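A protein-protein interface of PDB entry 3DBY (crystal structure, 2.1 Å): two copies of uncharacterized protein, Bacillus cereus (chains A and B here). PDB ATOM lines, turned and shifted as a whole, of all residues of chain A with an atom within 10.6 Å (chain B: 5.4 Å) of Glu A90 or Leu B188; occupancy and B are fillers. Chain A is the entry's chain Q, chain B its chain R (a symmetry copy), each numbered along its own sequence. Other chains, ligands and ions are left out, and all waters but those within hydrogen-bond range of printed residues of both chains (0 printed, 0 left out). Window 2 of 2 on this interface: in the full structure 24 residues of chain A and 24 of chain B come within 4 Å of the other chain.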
ATOM      1  N   GLU A  37     -18.641  14.897   4.112  1.00  0.00           N
ATOM      2  CA  GLU A  37     -17.302  15.002   4.705  1.00  0.00           C
ATOM      3  C   GLU A  37     -16.716  16.349   4.338  1.00  0.00           C
ATOM      4  O   GLU A  37     -15.685  16.407   3.671  1.00  0.00           O
ATOM      5  CB  GLU A  37     -16.411  13.870   4.154  1.00  0.00           C
ATOM      6  CG  GLU A  37     -16.929  12.491   4.545  1.00  0.00           C
ATOM      7  CD  GLU A  37     -16.699  12.161   6.035  1.00  0.00           C
ATOM      8  OE1 GLU A  37     -16.119  13.005   6.773  1.00  0.00           O
ATOM      9  OE2 GLU A  37     -17.100  11.049   6.454  1.00  0.00           O
ATOM     10  N   LEU A  82      -2.602   9.937   5.704  1.00  0.00           N
ATOM     11  CA  LEU A  82      -2.453   9.178   6.929  1.00  0.00           C
ATOM     12  C   LEU A  82      -3.594   9.508   7.880  1.00  0.00           C
ATOM     13  O   LEU A  82      -4.110   8.625   8.563  1.00  0.00           O
ATOM     14  CB  LEU A  82      -1.092   9.481   7.573  1.00  0.00           C
ATOM     15  CG  LEU A  82       0.089   8.851   6.826  1.00  0.00           C
ATOM     16  CD1 LEU A  82       1.427   9.238   7.448  1.00  0.00           C
ATOM     17  CD2 LEU A  82      -0.065   7.320   6.793  1.00  0.00           C
ATOM     18  N   ASN A  83      -4.016  10.770   7.921  1.00  0.00           N
ATOM     19  CA  ASN A  83      -5.183  11.118   8.750  1.00  0.00           C
ATOM     20  C   ASN A  83      -6.468  10.408   8.283  1.00  0.00           C
ATOM     21  O   ASN A  83      -7.302  10.012   9.093  1.00  0.00           O
ATOM     22  CB  ASN A  83      -5.447  12.617   8.801  1.00  0.00           C
ATOM     23  CG  ASN A  83      -6.485  12.980   9.861  1.00  0.00           C
ATOM     24  OD1 ASN A  83      -6.381  12.572  11.033  1.00  0.00           O
ATOM     25  ND2 ASN A  83      -7.507  13.718   9.457  1.00  0.00           N
ATOM     26  N   ILE A  84      -6.641  10.302   6.974  1.00  0.00           N
ATOM     27  CA  ILE A  84      -7.777   9.590   6.449  1.00  0.00           C
ATOM     28  C   ILE A  84      -7.731   8.105   6.875  1.00  0.00           C
ATOM     29  O   ILE A  84      -8.756   7.524   7.256  1.00  0.00           O
ATOM     30  CB  ILE A  84      -7.830   9.683   4.927  1.00  0.00           C
ATOM     31  CG1 ILE A  84      -8.125  11.136   4.517  1.00  0.00           C
ATOM     32  CG2 ILE A  84      -8.820   8.626   4.362  1.00  0.00           C
ATOM     33  CD1 ILE A  84      -8.169  11.359   3.022  1.00  0.00           C
ATOM     34  N   ILE A  85      -6.544   7.503   6.798  1.00  0.00           N
ATOM     35  CA  ILE A  85      -6.417   6.096   7.142  1.00  0.00           C
ATOM     36  C   ILE A  85      -6.699   5.947   8.625  1.00  0.00           C
ATOM     37  O   ILE A  85      -7.357   4.997   9.050  1.00  0.00           O
ATOM     38  CB  ILE A  85      -4.995   5.540   6.848  1.00  0.00           C
ATOM     39  CG1 ILE A  85      -4.788   5.397   5.317  1.00  0.00           C
ATOM     40  CG2 ILE A  85      -4.713   4.223   7.707  1.00  0.00           C
ATOM     41  CD1 ILE A  85      -3.370   5.074   4.916  1.00  0.00           C
ATOM     42  N   GLN A  86      -6.222   6.908   9.418  1.00  0.00           N
ATOM     43  CA  GLN A  86      -6.491   6.846  10.847  1.00  0.00           C
ATOM     44  C   GLN A  86      -7.988   6.830  11.118  1.00  0.00           C
ATOM     45  O   GLN A  86      -8.496   5.991  11.851  1.00  0.00           O
ATOM     46  CB  GLN A  86      -5.844   7.988  11.614  1.00  0.00           C
ATOM     47  CG  GLN A  86      -5.906   7.734  13.138  1.00  0.00           C
ATOM     48  CD  GLN A  86      -5.068   8.703  13.931  1.00  0.00           C
ATOM     49  OE1 GLN A  86      -5.615   9.581  14.610  1.00  0.00           O
ATOM     50  NE2 GLN A  86      -3.745   8.592  13.829  1.00  0.00           N
ATOM     51  N   LYS A  87      -8.699   7.740  10.488  1.00  0.00           N
ATOM     52  CA  LYS A  87     -10.135   7.776  10.650  1.00  0.00           C
ATOM     53  C   LYS A  87     -10.855   6.502  10.112  1.00  0.00           C
ATOM     54  O   LYS A  87     -11.899   6.124  10.610  1.00  0.00           O
ATOM     55  CB  LYS A  87     -10.677   9.089  10.068  1.00  0.00           C
ATOM     56  CG  LYS A  87     -10.320  10.241  11.014  1.00  0.00           C
ATOM     57  CD  LYS A  87     -10.655  11.665  10.567  1.00  0.00           C
ATOM     58  CE  LYS A  87     -11.480  11.745   9.329  1.00  0.00           C
ATOM     59  NZ  LYS A  87     -11.726  13.150   8.890  1.00  0.00           N
ATOM     60  N   GLN A  88     -10.294   5.844   9.106  1.00  0.00           N
ATOM     61  CA  GLN A  88     -10.905   4.627   8.587  1.00  0.00           C
ATOM     62  C   GLN A  88     -10.770   3.553   9.628  1.00  0.00           C
ATOM     63  O   GLN A  88     -11.714   2.850   9.923  1.00  0.00           O
ATOM     64  CB  GLN A  88     -10.229   4.179   7.290  1.00  0.00           C
ATOM     65  CG  GLN A  88     -10.540   5.085   6.073  1.00  0.00           C
ATOM     66  CD  GLN A  88      -9.761   4.675   4.809  1.00  0.00           C
ATOM     67  OE1 GLN A  88      -8.510   4.716   4.769  1.00  0.00           O
ATOM     68  NE2 GLN A  88     -10.494   4.250   3.784  1.00  0.00           N
ATOM     69  N   LEU A  89      -9.571   3.414  10.177  1.00  0.00           N
ATOM     70  CA  LEU A  89      -9.339   2.443  11.225  1.00  0.00           C
ATOM     71  C   LEU A  89     -10.148   2.698  12.489  1.00  0.00           C
ATOM     72  O   LEU A  89     -10.329   1.772  13.286  1.00  0.00           O
ATOM     73  CB  LEU A  89      -7.849   2.348  11.589  1.00  0.00           C
ATOM     74  CG  LEU A  89      -6.942   2.015  10.403  1.00  0.00           C
ATOM     75  CD1 LEU A  89      -5.485   2.050  10.815  1.00  0.00           C
ATOM     76  CD2 LEU A  89      -7.366   0.637   9.809  1.00  0.00           C
ATOM     77  N   GLU A  90     -10.656   3.918  12.671  1.00  0.00           N
ATOM     78  CA  GLU A  90     -11.484   4.231  13.870  1.00  0.00           C
ATOM     79  C   GLU A  90     -12.932   4.422  13.460  1.00  0.00           C
ATOM     80  O   GLU A  90     -13.722   4.888  14.255  1.00  0.00           O
ATOM     81  CB  GLU A  90     -11.044   5.538  14.541  1.00  0.00           C
ATOM     82  CG  GLU A  90      -9.742   5.467  15.334  1.00  0.00           C
ATOM     83  CD  GLU A  90      -9.080   6.845  15.477  1.00  0.00           C
ATOM     84  OE1 GLU A  90      -9.494   7.815  14.779  1.00  0.00           O
ATOM     85  OE2 GLU A  90      -8.128   6.962  16.283  1.00  0.00           O
ATOM     86  N   GLY A  91     -13.283   4.088  12.222  1.00  0.00           N
ATOM     87  CA  GLY A  91     -14.676   4.200  11.756  1.00  0.00           C
ATOM     88  C   GLY A  91     -15.187   5.633  11.754  1.00  0.00           C
ATOM     89  O   GLY A  91     -16.360   5.858  12.013  1.00  0.00           O
ATOM     90  N   LYS A  92     -14.328   6.607  11.421  1.00  0.00           N
ATOM     91  CA  LYS A  92     -14.714   8.010  11.565  1.00  0.00           C
ATOM     92  C   LYS A  92     -14.830   8.818  10.294  1.00  0.00           C
ATOM     93  O   LYS A  92     -14.834  10.063  10.360  1.00  0.00           O
ATOM     94  CB  LYS A  92     -13.742   8.759  12.504  1.00  0.00           C
ATOM     95  CG  LYS A  92     -13.980   8.493  13.986  1.00  0.00           C
ATOM     96  CD  LYS A  92     -12.835   8.997  14.869  1.00  0.00           C
ATOM     97  CE  LYS A  92     -13.347   9.064  16.319  1.00  0.00           C
ATOM     98  NZ  LYS A  92     -12.269   8.775  17.299  1.00  0.00           N
ATOM     99  N   ILE A  93     -14.880   8.161   9.143  1.00  0.00           N
ATOM    100  CA  ILE A  93     -14.985   8.867   7.860  1.00  0.00           C
ATOM    101  C   ILE A  93     -15.678   7.967   6.829  1.00  0.00           C
ATOM    102  O   ILE A  93     -15.468   6.770   6.839  1.00  0.00           O
ATOM    103  CB  ILE A  93     -13.608   9.267   7.265  1.00  0.00           C
ATOM    104  CG1 ILE A  93     -13.807  10.157   6.016  1.00  0.00           C
ATOM    105  CG2 ILE A  93     -12.805   8.020   6.830  1.00  0.00           C
ATOM    106  CD1 ILE A  93     -12.500  10.700   5.439  1.00  0.00           C
ATOM    107  N   THR A  94     -16.481   8.536   5.941  1.00  0.00           N
ATOM    108  CA  THR A  94     -16.993   7.753   4.846  1.00  0.00           C
ATOM    109  C   THR A  94     -16.233   8.152   3.570  1.00  0.00           C
ATOM    110  O   THR A  94     -16.337   9.298   3.089  1.00  0.00           O
ATOM    111  CB  THR A  94     -18.549   7.949   4.675  1.00  0.00           C
ATOM    112  OG1 THR A  94     -19.200   7.628   5.908  1.00  0.00           O
ATOM    113  CG2 THR A  94     -19.101   7.088   3.573  1.00  0.00           C
ATOM    114  N   ILE A  95     -15.447   7.221   3.032  1.00  0.00           N
ATOM    115  CA  ILE A  95     -14.697   7.484   1.797  1.00  0.00           C
ATOM    116  C   ILE A  95     -14.637   6.208   0.973  1.00  0.00           C
ATOM    117  O   ILE A  95     -14.431   5.135   1.522  1.00  0.00           O
ATOM    118  CB  ILE A  95     -13.253   8.033   2.090  1.00  0.00           C
ATOM    119  CG1 ILE A  95     -12.536   8.434   0.805  1.00  0.00           C
ATOM    120  CG2 ILE A  95     -12.389   7.034   2.866  1.00  0.00           C
ATOM    121  CD1 ILE A  95     -11.190   9.153   1.080  1.00  0.00           C
ATOM    122  N   PRO A  99      -8.592   1.178   3.116  1.00  0.00           N
ATOM    123  CA  PRO A  99      -7.332   1.649   3.706  1.00  0.00           C
ATOM    124  C   PRO A  99      -6.066   1.266   2.958  1.00  0.00           C
ATOM    125  O   PRO A  99      -5.137   2.072   2.897  1.00  0.00           O
ATOM    126  CB  PRO A  99      -7.340   1.027   5.112  1.00  0.00           C
ATOM    127  CG  PRO A  99      -8.769   0.904   5.430  1.00  0.00           C
ATOM    128  CD  PRO A  99      -9.436   0.510   4.130  1.00  0.00           C
ATOM    129  N   ASN A 103      -3.036   3.554   1.648  1.00  0.00           N
ATOM    130  CA  ASN A 103      -1.694   3.204   2.137  1.00  0.00           C
ATOM    131  C   ASN A 103      -0.644   3.190   0.984  1.00  0.00           C
ATOM    132  O   ASN A 103       0.529   3.611   1.134  1.00  0.00           O
ATOM    133  CB  ASN A 103      -1.734   1.884   2.925  1.00  0.00           C
ATOM    134  CG  ASN A 103      -0.452   1.592   3.698  1.00  0.00           C
ATOM    135  OD1 ASN A 103      -0.034   2.357   4.593  1.00  0.00           O
ATOM    136  ND2 ASN A 103       0.179   0.447   3.372  1.00  0.00           N
ATOM    137  N   TYR B 183       0.042   1.063   7.891  1.00  0.00           N
ATOM    138  CA  TYR B 183      -0.930   1.827   8.696  1.00  0.00           C
ATOM    139  C   TYR B 183      -0.324   2.414   9.986  1.00  0.00           C
ATOM    140  O   TYR B 183      -0.815   3.415  10.518  1.00  0.00           O
ATOM    141  CB  TYR B 183      -2.110   0.929   9.127  1.00  0.00           C
ATOM    142  CG  TYR B 183      -2.904   0.276   7.992  1.00  0.00           C
ATOM    143  CD1 TYR B 183      -2.666   0.581   6.636  1.00  0.00           C
ATOM    144  CD2 TYR B 183      -3.874  -0.664   8.281  1.00  0.00           C
ATOM    145  CE1 TYR B 183      -3.371  -0.088   5.596  1.00  0.00           C
ATOM    146  CE2 TYR B 183      -4.585  -1.301   7.276  1.00  0.00           C
ATOM    147  CZ  TYR B 183      -4.346  -1.030   5.959  1.00  0.00           C
ATOM    148  OH  TYR B 183      -5.119  -1.715   5.036  1.00  0.00           O
ATOM    149  N   LEU B 184       0.685   1.757  10.541  1.00  0.00           N
ATOM    150  CA  LEU B 184       1.337   2.302  11.723  1.00  0.00           C
ATOM    151  C   LEU B 184       1.948   3.711  11.523  1.00  0.00           C
ATOM    152  O   LEU B 184       2.307   4.372  12.479  1.00  0.00           O
ATOM    153  CB  LEU B 184       2.448   1.363  12.226  1.00  0.00           C
ATOM    154  CG  LEU B 184       2.171  -0.103  12.592  1.00  0.00           C
ATOM    155  CD1 LEU B 184       3.457  -0.739  13.246  1.00  0.00           C
ATOM    156  CD2 LEU B 184       0.995  -0.211  13.489  1.00  0.00           C
ATOM    157  N   THR B 186       0.365   6.123  10.679  1.00  0.00           N
ATOM    158  CA  THR B 186      -0.662   6.992  11.256  1.00  0.00           C
ATOM    159  C   THR B 186      -0.312   7.352  12.697  1.00  0.00           C
ATOM    160  O   THR B 186      -0.925   8.259  13.266  1.00  0.00           O
ATOM    161  CB  THR B 186      -2.083   6.340  11.297  1.00  0.00           C
ATOM    162  OG1 THR B 186      -2.052   5.188  12.115  1.00  0.00           O
ATOM    163  CG2 THR B 186      -2.541   5.886   9.941  1.00  0.00           C
ATOM    164  N   GLU B 187       0.654   6.648  13.284  1.00  0.00           N
ATOM    165  CA  GLU B 187       0.910   6.740  14.730  1.00  0.00           C
ATOM    166  C   GLU B 187      -0.168   6.131  15.678  1.00  0.00           C
ATOM    167  O   GLU B 187      -0.026   6.203  16.893  1.00  0.00           O
ATOM    168  CB  GLU B 187       1.272   8.186  15.159  1.00  0.00           C
ATOM    169  CG  GLU B 187       2.688   8.592  14.715  1.00  0.00           C
ATOM    170  CD  GLU B 187       2.922  10.112  14.785  1.00  0.00           C
ATOM    171  OE1 GLU B 187       2.630  10.819  13.784  1.00  0.00           O
ATOM    172  OE2 GLU B 187       3.397  10.598  15.847  1.00  0.00           O
ATOM    173  N   LEU B 188      -1.229   5.555  15.107  1.00  0.00           N
ATOM    174  CA  LEU B 188      -2.136   4.673  15.822  1.00  0.00           C
ATOM    175  C   LEU B 188      -1.526   3.303  15.752  1.00  0.00           C
ATOM    176  O   LEU B 188      -1.538   2.708  14.686  1.00  0.00           O
ATOM    177  CB  LEU B 188      -3.454   4.604  15.057  1.00  0.00           C
ATOM    178  CG  LEU B 188      -4.799   4.377  15.721  1.00  0.00           C
ATOM    179  CD1 LEU B 188      -5.046   5.534  16.714  1.00  0.00           C
ATOM    180  CD2 LEU B 188      -5.887   4.321  14.632  1.00  0.00           C
ATOM    181  N   HIS B 189      -1.024   2.773  16.869  1.00  0.00           N
ATOM    182  CA  HIS B 189      -0.269   1.511  16.853  1.00  0.00           C
ATOM    183  C   HIS B 189      -1.049   0.252  17.185  1.00  0.00           C
ATOM    184  O   HIS B 189      -0.599  -0.865  16.922  1.00  0.00           O
ATOM    185  CB  HIS B 189       1.014   1.658  17.678  1.00  0.00           C
ATOM    186  CG  HIS B 189       2.041   2.498  16.976  1.00  0.00           C
ATOM    187  ND1 HIS B 189       3.345   2.618  17.404  1.00  0.00           N
ATOM    188  CD2 HIS B 189       1.945   3.235  15.839  1.00  0.00           C
ATOM    189  CE1 HIS B 189       4.001   3.417  16.577  1.00  0.00           C
ATOM    190  NE2 HIS B 189       3.170   3.808  15.620  1.00  0.00           N
ATOM    191  N   HIS B 190      -2.233   0.443  17.749  1.00  0.00           N
ATOM    192  CA  HIS B 190      -3.106  -0.674  18.053  1.00  0.00           C
ATOM    193  C   HIS B 190      -4.468  -0.160  17.668  1.00  0.00           C
ATOM    194  O   HIS B 190      -4.793   1.018  17.932  1.00  0.00           O
ATOM    195  CB  HIS B 190      -3.003  -1.046  19.528  1.00  0.00           C
ATOM    196  CG  HIS B 190      -1.662  -1.618  19.888  1.00  0.00           C
ATOM    197  ND1 HIS B 190      -0.626  -0.841  20.361  1.00  0.00           N
ATOM    198  CD2 HIS B 190      -1.173  -2.877  19.786  1.00  0.00           C
ATOM    199  CE1 HIS B 190       0.438  -1.602  20.557  1.00  0.00           C
ATOM    200  NE2 HIS B 190       0.128  -2.844  20.218  1.00  0.00           N
ATOM    201  N   PHE B 191      -5.204  -0.976  16.938  1.00  0.00           N
ATOM    202  CA  PHE B 191      -6.493  -0.567  16.427  1.00  0.00           C
ATOM    203  C   PHE B 191      -7.181  -1.886  16.203  1.00  0.00           C
ATOM    204  O   PHE B 191      -6.512  -2.915  16.172  1.00  0.00           O
ATOM    205  CB  PHE B 191      -6.388   0.307  15.139  1.00  0.00           C
ATOM    206  CG  PHE B 191      -5.413  -0.228  14.097  1.00  0.00           C
ATOM    207  CD1 PHE B 191      -5.848  -1.080  13.082  1.00  0.00           C
ATOM    208  CD2 PHE B 191      -4.054   0.129  14.143  1.00  0.00           C
ATOM    209  CE1 PHE B 191      -4.952  -1.589  12.140  1.00  0.00           C
ATOM    210  CE2 PHE B 191      -3.167  -0.363  13.211  1.00  0.00           C
ATOM    211  CZ  PHE B 191      -3.613  -1.221  12.199  1.00  0.00           C
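Among the printed residues, merely in contact across the chains: Leu A82 with Thr B186 (3.4 Å), Ile A85 with Thr B186 (3.5 Å), Gln A86 with Leu B188 (3.7 Å), Leu A89 with Tyr B183 (3.9 Å), Leu A89 with Phe B191 (3.9 Å), Glu A90 with Leu B188 (3.4 Å), Pro A99 with Tyr B183 (3.5 Å) and Asn A103 with Tyr B183 (3.5 Å).
Glu A90 touches just one residue of chain B: Leu B188. Leu B188 touches just these residues of chain A: Gln A86 (3.7 Å) and Glu A90 (3.4 Å). No residue of chain A comes within 4 Å of Leu B184. No residue of chain A comes within 4 Å of His B189. Printed residues of chain B within 4 Å of Asn A103: Tyr B183. Of the printed residues of chain B, Leu A89 touches Tyr B183 and Phe B191. Printed residues of chain B within 4 Å of Gln A86: Thr B186 (2.9 Å) and Leu B188 (3.7 Å). Printed residues of chain B within 4 Å of Leu A82: Thr B186. Of the printed residues of chain A, Tyr B183 touches Leu A89, Pro A99 and Asn A103. Asn A83 touches none of the printed residues of chain B. The nearest printed residue of chain B that does not touch Glu A90 is Phe B191 (6.1 Å). The nearest residue of chain A that does not touch Leu B188 is Leu A89 (4.1 Å). The nearest printed residue of chain B that does not touch Asn A103 is Leu B184 (6.0 Å).
Of the 17 printed residues of chain A, 7 touch a printed residue of chain B. Printed residues of chain A that touch a printed residue of chain B: Leu A82, Ile A85, Gln A86, Leu A89, Glu A90, Pro A99 and Asn A103. Hydrophobic or aromatic side chains of chain A that line the printed part of chain B: Ile A85, Leu A89 and Pro A99. Hydrophobic or aromatic side chains of chain B within 4 Å of the printed part of chain A: Tyr B183, Leu B188 and Phe B191. Among the printed residues, 9 pairs touch across the chains.
No position is printed for both chains.
The side-chain carboxylate of Glu A90 lies within salt-bridge range of the side-chain amino group of Lys A92, at 3.9 Å. The backbone carbonyl oxygen of Tyr B183 is in hydrogen-bond range of the side-chain hydroxyl of Thr B186. OG1 of Thr B186 lies within hydrogen-bond range of N of Leu B188.
The side-chain amide nitrogen of Gln A86 lies within hydrogen-bond range of the backbone carbonyl oxygen of Thr B186 (2.9 Å).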
